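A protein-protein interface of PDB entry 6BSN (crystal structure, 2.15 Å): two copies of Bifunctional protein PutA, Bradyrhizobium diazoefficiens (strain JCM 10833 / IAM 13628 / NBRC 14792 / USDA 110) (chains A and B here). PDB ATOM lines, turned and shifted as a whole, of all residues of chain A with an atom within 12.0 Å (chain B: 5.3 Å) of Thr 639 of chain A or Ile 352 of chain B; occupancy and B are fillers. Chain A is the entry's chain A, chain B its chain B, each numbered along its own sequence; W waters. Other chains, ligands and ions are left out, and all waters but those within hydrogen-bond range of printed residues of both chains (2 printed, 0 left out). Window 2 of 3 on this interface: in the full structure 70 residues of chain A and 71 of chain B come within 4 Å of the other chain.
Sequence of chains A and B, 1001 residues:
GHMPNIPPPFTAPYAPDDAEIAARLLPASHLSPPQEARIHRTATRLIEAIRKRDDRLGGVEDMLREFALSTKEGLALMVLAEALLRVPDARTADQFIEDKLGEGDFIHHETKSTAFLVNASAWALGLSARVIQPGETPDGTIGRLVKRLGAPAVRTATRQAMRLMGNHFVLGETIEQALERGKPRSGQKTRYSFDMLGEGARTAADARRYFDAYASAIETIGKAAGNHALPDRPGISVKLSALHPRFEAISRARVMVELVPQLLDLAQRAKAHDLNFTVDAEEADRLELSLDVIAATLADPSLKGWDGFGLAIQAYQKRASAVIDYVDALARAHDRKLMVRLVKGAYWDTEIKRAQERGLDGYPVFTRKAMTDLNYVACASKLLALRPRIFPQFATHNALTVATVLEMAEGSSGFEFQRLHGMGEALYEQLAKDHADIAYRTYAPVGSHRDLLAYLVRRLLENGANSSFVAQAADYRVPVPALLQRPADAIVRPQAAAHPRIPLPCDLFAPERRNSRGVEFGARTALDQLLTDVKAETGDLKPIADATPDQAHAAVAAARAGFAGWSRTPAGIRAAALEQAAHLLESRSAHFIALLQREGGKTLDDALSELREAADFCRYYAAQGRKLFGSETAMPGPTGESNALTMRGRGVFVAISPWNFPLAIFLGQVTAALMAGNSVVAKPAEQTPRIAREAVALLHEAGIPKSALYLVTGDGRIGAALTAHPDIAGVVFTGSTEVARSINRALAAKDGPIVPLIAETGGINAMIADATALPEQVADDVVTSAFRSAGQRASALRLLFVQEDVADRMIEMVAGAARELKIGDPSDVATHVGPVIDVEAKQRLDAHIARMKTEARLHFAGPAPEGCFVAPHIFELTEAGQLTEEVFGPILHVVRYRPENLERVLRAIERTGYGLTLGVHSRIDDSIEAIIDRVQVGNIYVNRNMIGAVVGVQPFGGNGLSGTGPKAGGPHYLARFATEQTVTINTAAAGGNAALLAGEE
The backbone carbonyl oxygen (O) of Gly 640 of chain A sits at hydrogen-bond distance from the side-chain amino group (NZ) of Lys 353 of chain B (2.9 Å). OE1 of Gln 356 of chain B lies within hydrogen-bond range of N of Thr 639 of chain A (2.7 Å). The side-chain amide oxygen of Asn 986 of chain A lies within hydrogen-bond range of the side-chain amino group of Lys 353 of chain B.
The side-chain amide oxygen of Asn 986 of chain A lies within hydrogen-bond range of the backbone NH of Ala 988 of chain A (3.0 Å). O of Gly 640 of chain A lies close to OD1 of Asn 986 of chain A (3.4 Å). The backbone NH (N) of Thr 987 of chain A lies within hydrogen-bond range of the backbone carbonyl oxygen (O) of Gly 640 of chain A. The side-chain hydroxyl (OH) of Tyr 363 of chain B sits at hydrogen-bond distance from the side-chain amide nitrogen (NE2) of Gln 356 of chain B (3.0 Å). The backbone carbonyl oxygen (O) of Gly 640 of chain A is in hydrogen-bond range of the backbone NH (N) of Ala 988 of chain A (3.3 Å).
Pro 638 of chain A touches Gln 356 of chain B (CA to OE1, 3.2 Å). Pro 638 of chain A touches Glu 357 of chain B (CB to CG, 3.95 Å). CG2 of Ile 352 of chain B touches CG2 of Thr 639 of chain A (3.6 Å). Thr 639 of chain A touches Lys 353 of chain B (O to CD, 3.2 Å).
Thr 639 of chain A touches three residues of chain B. Of the printed residues of chain A, Ile 352 of chain B touches Thr 639 (3.6 Å). No residue of chain A comes within 4 Å of Asp 349 of chain B. No residue of chain A comes within 4 Å of Thr 350 of chain B. No residue of chain A comes within 4 Å of Glu 351 of chain B. Of chain A, only Thr 639, Gly 640 and Asn 986 come within 4 Å of Lys 353 of chain B. No residue of chain A comes within 4 Å of Ala 355 of chain B. Gln 356 of chain B touches just these residues of chain A: Pro 638 and Thr 639. Val 365 of chain B touches none of the printed residues of chain A. No residue of chain A comes within 4 Å of Thr 367 of chain B. Of the printed residues of chain A, Glu 357 of chain B touches Pro 638. Of the printed residues of chain B, Gly 640 of chain A touches Lys 353 (2.9 Å). Phe 366 of chain B touches none of the printed residues of chain A. Ala 988 of chain A touches none of the printed residues of chain B. The nearest residue of chain A that does not touch Ile 352 of chain B is Pro 638 of chain A (6.4 Å). The nearest printed residue of chain B that does not touch Gly 640 of chain A is Gln 356 of chain B (6.0 Å).
Hydrophobic or aromatic side chains of chain A within 4 Å of the printed part of chain B: Pro 638. Along chain A the printed residues that touch a printed residue of chain B span positions 638 to 986. Hydrophobic or aromatic side chains of chain B that line the printed part of chain A: Ile 352.
No position is printed for both chains.
Water W1 bridges OE2 of Glu 357 of chain B and OE1 of Glu 641 of chain A. Water W2 bridges OE1 of Glu 641 of chain A (2.7 Å) and NZ of Lys 353 of chain B (2.7 Å).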
ATOM      1  N   MET A 635     -17.108 -26.727  32.604  1.00  0.00           N
ATOM      2  CA  MET A 635     -17.837 -27.662  31.774  1.00  0.00           C
ATOM      3  C   MET A 635     -16.861 -28.389  30.864  1.00  0.00           C
ATOM      4  O   MET A 635     -15.845 -27.816  30.455  1.00  0.00           O
ATOM      5  CB  MET A 635     -18.904 -26.957  30.916  1.00  0.00           C
ATOM      6  CG  MET A 635     -19.883 -26.054  31.671  1.00  0.00           C
ATOM      7  SD  MET A 635     -20.844 -26.853  32.971  1.00  0.00           S
ATOM      8  CE  MET A 635     -21.859 -27.929  32.004  1.00  0.00           C
ATOM      9  N   PRO A 636     -17.102 -29.661  30.552  1.00  0.00           N
ATOM     10  CA  PRO A 636     -16.228 -30.344  29.603  1.00  0.00           C
ATOM     11  C   PRO A 636     -16.443 -29.747  28.232  1.00  0.00           C
ATOM     12  O   PRO A 636     -17.451 -29.098  27.955  1.00  0.00           O
ATOM     13  CB  PRO A 636     -16.699 -31.797  29.663  1.00  0.00           C
ATOM     14  CG  PRO A 636     -18.192 -31.632  29.888  1.00  0.00           C
ATOM     15  CD  PRO A 636     -18.318 -30.451  30.830  1.00  0.00           C
ATOM     16  N   GLY A 637     -15.481 -29.953  27.368  1.00  0.00           N
ATOM     17  CA  GLY A 637     -15.618 -29.418  26.048  1.00  0.00           C
ATOM     18  C   GLY A 637     -14.355 -29.559  25.261  1.00  0.00           C
ATOM     19  O   GLY A 637     -13.386 -30.186  25.688  1.00  0.00           O
ATOM     20  N   PRO A 638     -14.340 -28.954  24.087  1.00  0.00           N
ATOM     21  CA  PRO A 638     -13.196 -29.117  23.208  1.00  0.00           C
ATOM     22  C   PRO A 638     -12.000 -28.422  23.814  1.00  0.00           C
ATOM     23  O   PRO A 638     -12.124 -27.562  24.688  1.00  0.00           O
ATOM     24  CB  PRO A 638     -13.647 -28.452  21.907  1.00  0.00           C
ATOM     25  CG  PRO A 638     -14.621 -27.414  22.359  1.00  0.00           C
ATOM     26  CD  PRO A 638     -15.299 -27.953  23.588  1.00  0.00           C
ATOM     27  N   THR A 639     -10.833 -28.849  23.374  1.00  0.00           N
ATOM     28  CA  THR A 639      -9.613 -28.165  23.750  1.00  0.00           C
ATOM     29  C   THR A 639      -9.570 -26.783  23.080  1.00  0.00           C
ATOM     30  O   THR A 639     -10.303 -26.512  22.126  1.00  0.00           O
ATOM     31  CB  THR A 639      -8.408 -29.031  23.373  1.00  0.00           C
ATOM     32  OG1 THR A 639      -7.233 -28.544  24.027  1.00  0.00           O
ATOM     33  CG2 THR A 639      -8.184 -29.011  21.865  1.00  0.00           C
ATOM     34  N   GLY A 640      -8.733 -25.890  23.619  1.00  0.00           N
ATOM     35  CA  GLY A 640      -8.658 -24.523  23.128  1.00  0.00           C
ATOM     36  C   GLY A 640      -9.842 -23.632  23.481  1.00  0.00           C
ATOM     37  O   GLY A 640     -10.044 -22.597  22.834  1.00  0.00           O
ATOM     38  N   GLU A 641     -10.637 -24.003  24.482  1.00  0.00           N
ATOM     39  CA  GLU A 641     -11.840 -23.257  24.829  1.00  0.00           C
ATOM     40  C   GLU A 641     -12.212 -23.591  26.258  1.00  0.00           C
ATOM     41  O   GLU A 641     -12.293 -24.768  26.607  1.00  0.00           O
ATOM     42  CB  GLU A 641     -13.015 -23.602  23.881  1.00  0.00           C
ATOM     43  CG  GLU A 641     -14.333 -22.936  24.252  1.00  0.00           C
ATOM     44  CD  GLU A 641     -15.496 -23.348  23.351  1.00  0.00           C
ATOM     45  OE1 GLU A 641     -15.675 -22.707  22.284  1.00  0.00           O
ATOM     46  OE2 GLU A 641     -16.229 -24.308  23.700  1.00  0.00           O
ATOM     47  N   SER A 642     -12.485 -22.571  27.065  1.00  0.00           N
ATOM     48  CA  SER A 642     -12.939 -22.792  28.432  1.00  0.00           C
ATOM     49  C   SER A 642     -14.403 -22.397  28.564  1.00  0.00           C
ATOM     50  O   SER A 642     -14.851 -21.407  27.971  1.00  0.00           O
ATOM     51  CB  SER A 642     -12.100 -22.008  29.446  1.00  0.00           C
ATOM     52  OG  SER A 642     -12.406 -20.625  29.402  1.00  0.00           O
ATOM     53  N   ASN A 643     -15.134 -23.167  29.370  1.00  0.00           N
ATOM     54  CA  ASN A 643     -16.556 -22.968  29.605  1.00  0.00           C
ATOM     55  C   ASN A 643     -16.811 -23.052  31.098  1.00  0.00           C
ATOM     56  O   ASN A 643     -16.511 -24.074  31.717  1.00  0.00           O
ATOM     57  CB  ASN A 643     -17.385 -24.006  28.848  1.00  0.00           C
ATOM     58  CG  ASN A 643     -17.304 -23.819  27.359  1.00  0.00           C
ATOM     59  OD1 ASN A 643     -18.104 -23.078  26.792  1.00  0.00           O
ATOM     60  ND2 ASN A 643     -16.329 -24.468  26.710  1.00  0.00           N
ATOM     61  N   THR A 984     -17.846 -18.492  27.891  1.00  0.00           N
ATOM     62  CA  THR A 984     -17.130 -19.318  26.934  1.00  0.00           C
ATOM     63  C   THR A 984     -16.031 -18.471  26.326  1.00  0.00           C
ATOM     64  O   THR A 984     -16.320 -17.475  25.664  1.00  0.00           O
ATOM     65  CB  THR A 984     -18.068 -19.794  25.830  1.00  0.00           C
ATOM     66  OG1 THR A 984     -19.152 -20.486  26.422  1.00  0.00           O
ATOM     67  CG2 THR A 984     -17.347 -20.687  24.827  1.00  0.00           C
ATOM     68  N   ILE A 985     -14.783 -18.875  26.529  1.00  0.00           N
ATOM     69  CA  ILE A 985     -13.629 -18.125  26.067  1.00  0.00           C
ATOM     70  C   ILE A 985     -12.860 -18.989  25.084  1.00  0.00           C
ATOM     71  O   ILE A 985     -12.436 -20.091  25.427  1.00  0.00           O
ATOM     72  CB  ILE A 985     -12.719 -17.705  27.230  1.00  0.00           C
ATOM     73  CG1 ILE A 985     -13.524 -16.927  28.258  1.00  0.00           C
ATOM     74  CG2 ILE A 985     -11.512 -16.870  26.693  1.00  0.00           C
ATOM     75  CD1 ILE A 985     -12.760 -16.583  29.483  1.00  0.00           C
ATOM     76  N   ASN A 986     -12.649 -18.481  23.878  1.00  0.00           N
ATOM     77  CA  ASN A 986     -11.787 -19.165  22.927  1.00  0.00           C
ATOM     78  C   ASN A 986     -10.348 -18.879  23.355  1.00  0.00           C
ATOM     79  O   ASN A 986      -9.818 -17.802  23.106  1.00  0.00           O
ATOM     80  CB  ASN A 986     -12.101 -18.717  21.505  1.00  0.00           C
ATOM     81  CG  ASN A 986     -11.017 -19.085  20.517  1.00  0.00           C
ATOM     82  OD1 ASN A 986     -10.145 -19.894  20.801  1.00  0.00           O
ATOM     83  ND2 ASN A 986     -11.088 -18.506  19.327  1.00  0.00           N
ATOM     84  N   THR A 987      -9.720 -19.846  24.018  1.00  0.00           N
ATOM     85  CA  THR A 987      -8.388 -19.659  24.575  1.00  0.00           C
ATOM     86  C   THR A 987      -7.287 -19.991  23.578  1.00  0.00           C
ATOM     87  O   THR A 987      -6.110 -19.870  23.925  1.00  0.00           O
ATOM     88  CB  THR A 987      -8.212 -20.509  25.865  1.00  0.00           C
ATOM     89  OG1 THR A 987      -8.477 -21.887  25.595  1.00  0.00           O
ATOM     90  CG2 THR A 987      -9.175 -20.076  26.952  1.00  0.00           C
ATOM     91  N   ALA A 988      -7.639 -20.352  22.339  1.00  0.00           N
ATOM     92  CA  ALA A 988      -6.653 -20.907  21.413  1.00  0.00           C
ATOM     93  C   ALA A 988      -5.541 -19.925  21.074  1.00  0.00           C
ATOM     94  O   ALA A 988      -4.420 -20.355  20.770  1.00  0.00           O
ATOM     95  CB  ALA A 988      -7.330 -21.385  20.132  1.00  0.00           C
ATOM     96  N   ALA A 989      -5.816 -18.613  21.121  1.00  0.00           N
ATOM     97  CA  ALA A 989      -4.769 -17.622  20.862  1.00  0.00           C
ATOM     98  C   ALA A 989      -3.547 -17.833  21.756  1.00  0.00           C
ATOM     99  O   ALA A 989      -2.413 -17.566  21.335  1.00  0.00           O
ATOM    100  CB  ALA A 989      -5.325 -16.206  21.043  1.00  0.00           C
ATOM    101  N   ALA A 990      -3.760 -18.322  22.979  1.00  0.00           N
ATOM    102  CA  ALA A 990      -2.685 -18.628  23.926  1.00  0.00           C
ATOM    103  C   ALA A 990      -2.198 -20.070  23.777  1.00  0.00           C
ATOM    104  O   ALA A 990      -1.203 -20.466  24.386  1.00  0.00           O
ATOM    105  CB  ALA A 990      -3.154 -18.379  25.361  1.00  0.00           C
ATOM    106  N   TYR B 347      -0.604 -25.964  12.108  1.00  0.00           N
ATOM    107  CA  TYR B 347      -1.976 -25.829  12.587  1.00  0.00           C
ATOM    108  C   TYR B 347      -2.373 -26.947  13.554  1.00  0.00           C
ATOM    109  O   TYR B 347      -3.549 -27.317  13.606  1.00  0.00           O
ATOM    110  CB  TYR B 347      -2.956 -25.800  11.409  1.00  0.00           C
ATOM    111  CG  TYR B 347      -2.617 -24.767  10.357  1.00  0.00           C
ATOM    112  CD1 TYR B 347      -1.678 -25.028   9.370  1.00  0.00           C
ATOM    113  CD2 TYR B 347      -3.228 -23.518  10.364  1.00  0.00           C
ATOM    114  CE1 TYR B 347      -1.369 -24.078   8.413  1.00  0.00           C
ATOM    115  CE2 TYR B 347      -2.929 -22.564   9.408  1.00  0.00           C
ATOM    116  CZ  TYR B 347      -2.002 -22.846   8.437  1.00  0.00           C
ATOM    117  OH  TYR B 347      -1.698 -21.887   7.493  1.00  0.00           O
ATOM    118  N   TRP B 348      -1.417 -27.506  14.320  1.00  0.00           N
ATOM    119  CA  TRP B 348      -1.715 -28.684  15.150  1.00  0.00           C
ATOM    120  C   TRP B 348      -2.869 -28.420  16.118  1.00  0.00           C
ATOM    121  O   TRP B 348      -3.834 -29.192  16.177  1.00  0.00           O
ATOM    122  CB  TRP B 348      -0.468 -29.152  15.917  1.00  0.00           C
ATOM    123  CG  TRP B 348      -0.692 -30.443  16.670  1.00  0.00           C
ATOM    124  CD1 TRP B 348      -0.591 -31.705  16.166  1.00  0.00           C
ATOM    125  CD2 TRP B 348      -1.100 -30.593  18.046  1.00  0.00           C
ATOM    126  NE1 TRP B 348      -0.925 -32.632  17.129  1.00  0.00           N
ATOM    127  CE2 TRP B 348      -1.219 -31.982  18.297  1.00  0.00           C
ATOM    128  CE3 TRP B 348      -1.365 -29.692  19.089  1.00  0.00           C
ATOM    129  CZ2 TRP B 348      -1.578 -32.499  19.557  1.00  0.00           C
ATOM    130  CZ3 TRP B 348      -1.729 -30.207  20.346  1.00  0.00           C
ATOM    131  CH2 TRP B 348      -1.827 -31.597  20.565  1.00  0.00           C
ATOM    132  N   ASP B 349      -2.785 -27.336  16.896  1.00  0.00           N
ATOM    133  CA  ASP B 349      -3.837 -27.059  17.872  1.00  0.00           C
ATOM    134  C   ASP B 349      -5.182 -26.875  17.193  1.00  0.00           C
ATOM    135  O   ASP B 349      -6.207 -27.323  17.711  1.00  0.00           O
ATOM    136  CB  ASP B 349      -3.493 -25.827  18.703  1.00  0.00           C
ATOM    137  CG  ASP B 349      -2.239 -26.022  19.520  1.00  0.00           C
ATOM    138  OD1 ASP B 349      -2.315 -26.708  20.555  1.00  0.00           O
ATOM    139  OD2 ASP B 349      -1.174 -25.520  19.110  1.00  0.00           O
ATOM    140  N   THR B 350      -5.197 -26.208  16.035  1.00  0.00           N
ATOM    141  CA  THR B 350      -6.445 -26.026  15.299  1.00  0.00           C
ATOM    142  C   THR B 350      -7.027 -27.362  14.870  1.00  0.00           C
ATOM    143  O   THR B 350      -8.230 -27.601  15.010  1.00  0.00           O
ATOM    144  CB  THR B 350      -6.232 -25.121  14.084  1.00  0.00           C
ATOM    145  OG1 THR B 350      -5.907 -23.804  14.526  1.00  0.00           O
ATOM    146  CG2 THR B 350      -7.500 -25.048  13.266  1.00  0.00           C
ATOM    147  N   GLU B 351      -6.191 -28.252  14.339  1.00  0.00           N
ATOM    148  CA  GLU B 351      -6.716 -29.539  13.894  1.00  0.00           C
ATOM    149  C   GLU B 351      -7.321 -30.334  15.050  1.00  0.00           C
ATOM    150  O   GLU B 351      -8.371 -30.964  14.877  1.00  0.00           O
ATOM    151  CB  GLU B 351      -5.631 -30.346  13.183  1.00  0.00           C
ATOM    152  CG  GLU B 351      -4.955 -29.641  11.990  1.00  0.00           C
ATOM    153  CD  GLU B 351      -5.907 -29.321  10.874  1.00  0.00           C
ATOM    154  OE1 GLU B 351      -7.067 -29.769  10.943  1.00  0.00           O
ATOM    155  OE2 GLU B 351      -5.497 -28.631   9.906  1.00  0.00           O
ATOM    156  N   ILE B 352      -6.678 -30.325  16.229  1.00  0.00           N
ATOM    157  CA  ILE B 352      -7.222 -31.048  17.386  1.00  0.00           C
ATOM    158  C   ILE B 352      -8.583 -30.482  17.765  1.00  0.00           C
ATOM    159  O   ILE B 352      -9.583 -31.205  17.839  1.00  0.00           O
ATOM    160  CB  ILE B 352      -6.255 -30.986  18.586  1.00  0.00           C
ATOM    161  CG1 ILE B 352      -4.902 -31.626  18.252  1.00  0.00           C
ATOM    162  CG2 ILE B 352      -6.887 -31.675  19.827  1.00  0.00           C
ATOM    163  CD1 ILE B 352      -5.002 -32.984  17.655  1.00  0.00           C
ATOM    164  N   LYS B 353      -8.630 -29.173  18.016  1.00  0.00           N
ATOM    165  CA  LYS B 353      -9.880 -28.513  18.384  1.00  0.00           C
ATOM    166  C   LYS B 353     -10.967 -28.767  17.342  1.00  0.00           C
ATOM    167  O   LYS B 353     -12.103 -29.116  17.683  1.00  0.00           O
ATOM    168  CB  LYS B 353      -9.631 -27.010  18.558  1.00  0.00           C
ATOM    169  CG  LYS B 353     -10.873 -26.222  18.974  1.00  0.00           C
ATOM    170  CD  LYS B 353     -10.508 -24.824  19.410  1.00  0.00           C
ATOM    171  CE  LYS B 353     -11.687 -24.120  20.062  1.00  0.00           C
ATOM    172  NZ  LYS B 353     -11.404 -22.648  20.260  1.00  0.00           N
ATOM    173  N   ARG B 354     -10.632 -28.606  16.055  1.00  0.00           N
ATOM    174  CA  ARG B 354     -11.640 -28.782  15.011  1.00  0.00           C
ATOM    175  C   ARG B 354     -12.198 -30.196  15.010  1.00  0.00           C
ATOM    176  O   ARG B 354     -13.409 -30.393  14.860  1.00  0.00           O
ATOM    177  CB  ARG B 354     -11.058 -28.466  13.636  1.00  0.00           C
ATOM    178  CG  ARG B 354     -11.069 -27.006  13.281  1.00  0.00           C
ATOM    179  CD  ARG B 354     -10.274 -26.789  12.003  1.00  0.00           C
ATOM    180  NE  ARG B 354     -10.258 -25.386  11.595  1.00  0.00           N
ATOM    181  CZ  ARG B 354     -10.103 -24.985  10.337  1.00  0.00           C
ATOM    182  NH1 ARG B 354     -10.115 -23.691  10.050  1.00  0.00           N
ATOM    183  NH2 ARG B 354      -9.946 -25.880   9.369  1.00  0.00           N
ATOM    184  N   ALA B 355     -11.330 -31.200  15.143  1.00  0.00           N
ATOM    185  CA  ALA B 355     -11.828 -32.572  15.118  1.00  0.00           C
ATOM    186  C   ALA B 355     -12.769 -32.828  16.290  1.00  0.00           C
ATOM    187  O   ALA B 355     -13.789 -33.506  16.137  1.00  0.00           O
ATOM    188  CB  ALA B 355     -10.668 -33.564  15.115  1.00  0.00           C
ATOM    189  N   GLN B 356     -12.463 -32.260  17.459  1.00  0.00           N
ATOM    190  CA  GLN B 356     -13.326 -32.436  18.626  1.00  0.00           C
ATOM    191  C   GLN B 356     -14.674 -31.764  18.417  1.00  0.00           C
ATOM    192  O   GLN B 356     -15.722 -32.406  18.567  1.00  0.00           O
ATOM    193  CB  GLN B 356     -12.630 -31.898  19.876  1.00  0.00           C
ATOM    194  CG  GLN B 356     -11.308 -32.597  20.150  1.00  0.00           C
ATOM    195  CD  GLN B 356     -10.686 -32.190  21.461  1.00  0.00           C
ATOM    196  OE1 GLN B 356     -11.098 -31.205  22.078  1.00  0.00           O
ATOM    197  NE2 GLN B 356      -9.685 -32.947  21.902  1.00  0.00           N
ATOM    198  N   GLU B 357     -14.660 -30.478  18.036  1.00  0.00           N
ATOM    199  CA  GLU B 357     -15.890 -29.735  17.781  1.00  0.00           C
ATOM    200  C   GLU B 357     -16.751 -30.431  16.741  1.00  0.00           C
ATOM    201  O   GLU B 357     -17.981 -30.496  16.877  1.00  0.00           O
ATOM    202  CB  GLU B 357     -15.565 -28.315  17.289  1.00  0.00           C
ATOM    203  CG  GLU B 357     -14.803 -27.425  18.270  1.00  0.00           C
ATOM    204  CD  GLU B 357     -14.401 -26.072  17.657  1.00  0.00           C
ATOM    205  OE1 GLU B 357     -14.035 -26.034  16.463  1.00  0.00           O
ATOM    206  OE2 GLU B 357     -14.439 -25.046  18.374  1.00  0.00           O
ATOM    207  N   TYR B 363      -8.352 -37.903  14.520  1.00  0.00           N
ATOM    208  CA  TYR B 363      -7.620 -36.690  14.181  1.00  0.00           C
ATOM    209  C   TYR B 363      -6.855 -36.895  12.888  1.00  0.00           C
ATOM    210  O   TYR B 363      -6.188 -37.930  12.735  1.00  0.00           O
ATOM    211  CB  TYR B 363      -6.647 -36.330  15.299  1.00  0.00           C
ATOM    212  CG  TYR B 363      -7.332 -36.088  16.622  1.00  0.00           C
ATOM    213  CD1 TYR B 363      -7.362 -37.079  17.612  1.00  0.00           C
ATOM    214  CD2 TYR B 363      -7.973 -34.875  16.877  1.00  0.00           C
ATOM    215  CE1 TYR B 363      -8.010 -36.850  18.830  1.00  0.00           C
ATOM    216  CE2 TYR B 363      -8.596 -34.635  18.081  1.00  0.00           C
ATOM    217  CZ  TYR B 363      -8.617 -35.630  19.057  1.00  0.00           C
ATOM    218  OH  TYR B 363      -9.258 -35.378  20.248  1.00  0.00           O
ATOM    219  N   VAL B 365      -4.210 -35.425  12.184  1.00  0.00           N
ATOM    220  CA  VAL B 365      -2.802 -35.275  12.525  1.00  0.00           C
ATOM    221  C   VAL B 365      -2.454 -36.275  13.617  1.00  0.00           C
ATOM    222  O   VAL B 365      -3.313 -36.731  14.373  1.00  0.00           O
ATOM    223  CB  VAL B 365      -2.452 -33.847  12.991  1.00  0.00           C
ATOM    224  CG1 VAL B 365      -2.531 -32.852  11.836  1.00  0.00           C
ATOM    225  CG2 VAL B 365      -3.361 -33.441  14.133  1.00  0.00           C
ATOM    226  N   PHE B 366      -1.162 -36.594  13.717  1.00  0.00           N
ATOM    227  CA  PHE B 366      -0.678 -37.298  14.893  1.00  0.00           C
ATOM    228  C   PHE B 366      -0.868 -36.421  16.118  1.00  0.00           C
ATOM    229  O   PHE B 366      -0.983 -35.188  16.023  1.00  0.00           O
ATOM    230  CB  PHE B 366       0.793 -37.673  14.740  1.00  0.00           C
ATOM    231  CG  PHE B 366       1.064 -38.489  13.510  1.00  0.00           C
ATOM    232  CD1 PHE B 366       0.627 -39.807  13.426  1.00  0.00           C
ATOM    233  CD2 PHE B 366       1.696 -37.918  12.409  1.00  0.00           C
ATOM    234  CE1 PHE B 366       0.846 -40.553  12.280  1.00  0.00           C
ATOM    235  CE2 PHE B 366       1.923 -38.659  11.268  1.00  0.00           C
ATOM    236  CZ  PHE B 366       1.499 -39.974  11.198  1.00  0.00           C
ATOM    237  N   THR B 367      -0.947 -37.083  17.275  1.00  0.00           N
ATOM    238  CA  THR B 367      -1.137 -36.427  18.560  1.00  0.00           C
ATOM    239  C   THR B 367       0.081 -36.539  19.469  1.00  0.00           C
ATOM    240  O   THR B 367       0.082 -35.952  20.551  1.00  0.00           O
ATOM    241  CB  THR B 367      -2.376 -36.996  19.270  1.00  0.00           C
ATOM    242  OG1 THR B 367      -2.292 -38.430  19.318  1.00  0.00           O
ATOM    243  CG2 THR B 367      -3.671 -36.584  18.529  1.00  0.00           C
ATOM    244  N   ILE B 502      -5.208 -37.297  25.196  1.00  0.00           N
ATOM    245  CA  ILE B 502      -6.070 -36.638  24.224  1.00  0.00           C
ATOM    246  C   ILE B 502      -7.089 -37.658  23.739  1.00  0.00           C
ATOM    247  O   ILE B 502      -6.768 -38.539  22.937  1.00  0.00           O
ATOM    248  CB  ILE B 502      -5.266 -36.050  23.047  1.00  0.00           C
ATOM    249  CG1 ILE B 502      -4.261 -35.019  23.568  1.00  0.00           C
ATOM    250  CG2 ILE B 502      -6.201 -35.346  22.071  1.00  0.00           C
ATOM    251  CD1 ILE B 502      -3.432 -34.369  22.483  1.00  0.00           C
HETATM  252  O   HOH W   1     -15.914 -24.021  20.019  1.00  0.00           O
HETATM  253  O   HOH W   2     -13.718 -21.358  20.971  1.00  0.00           O
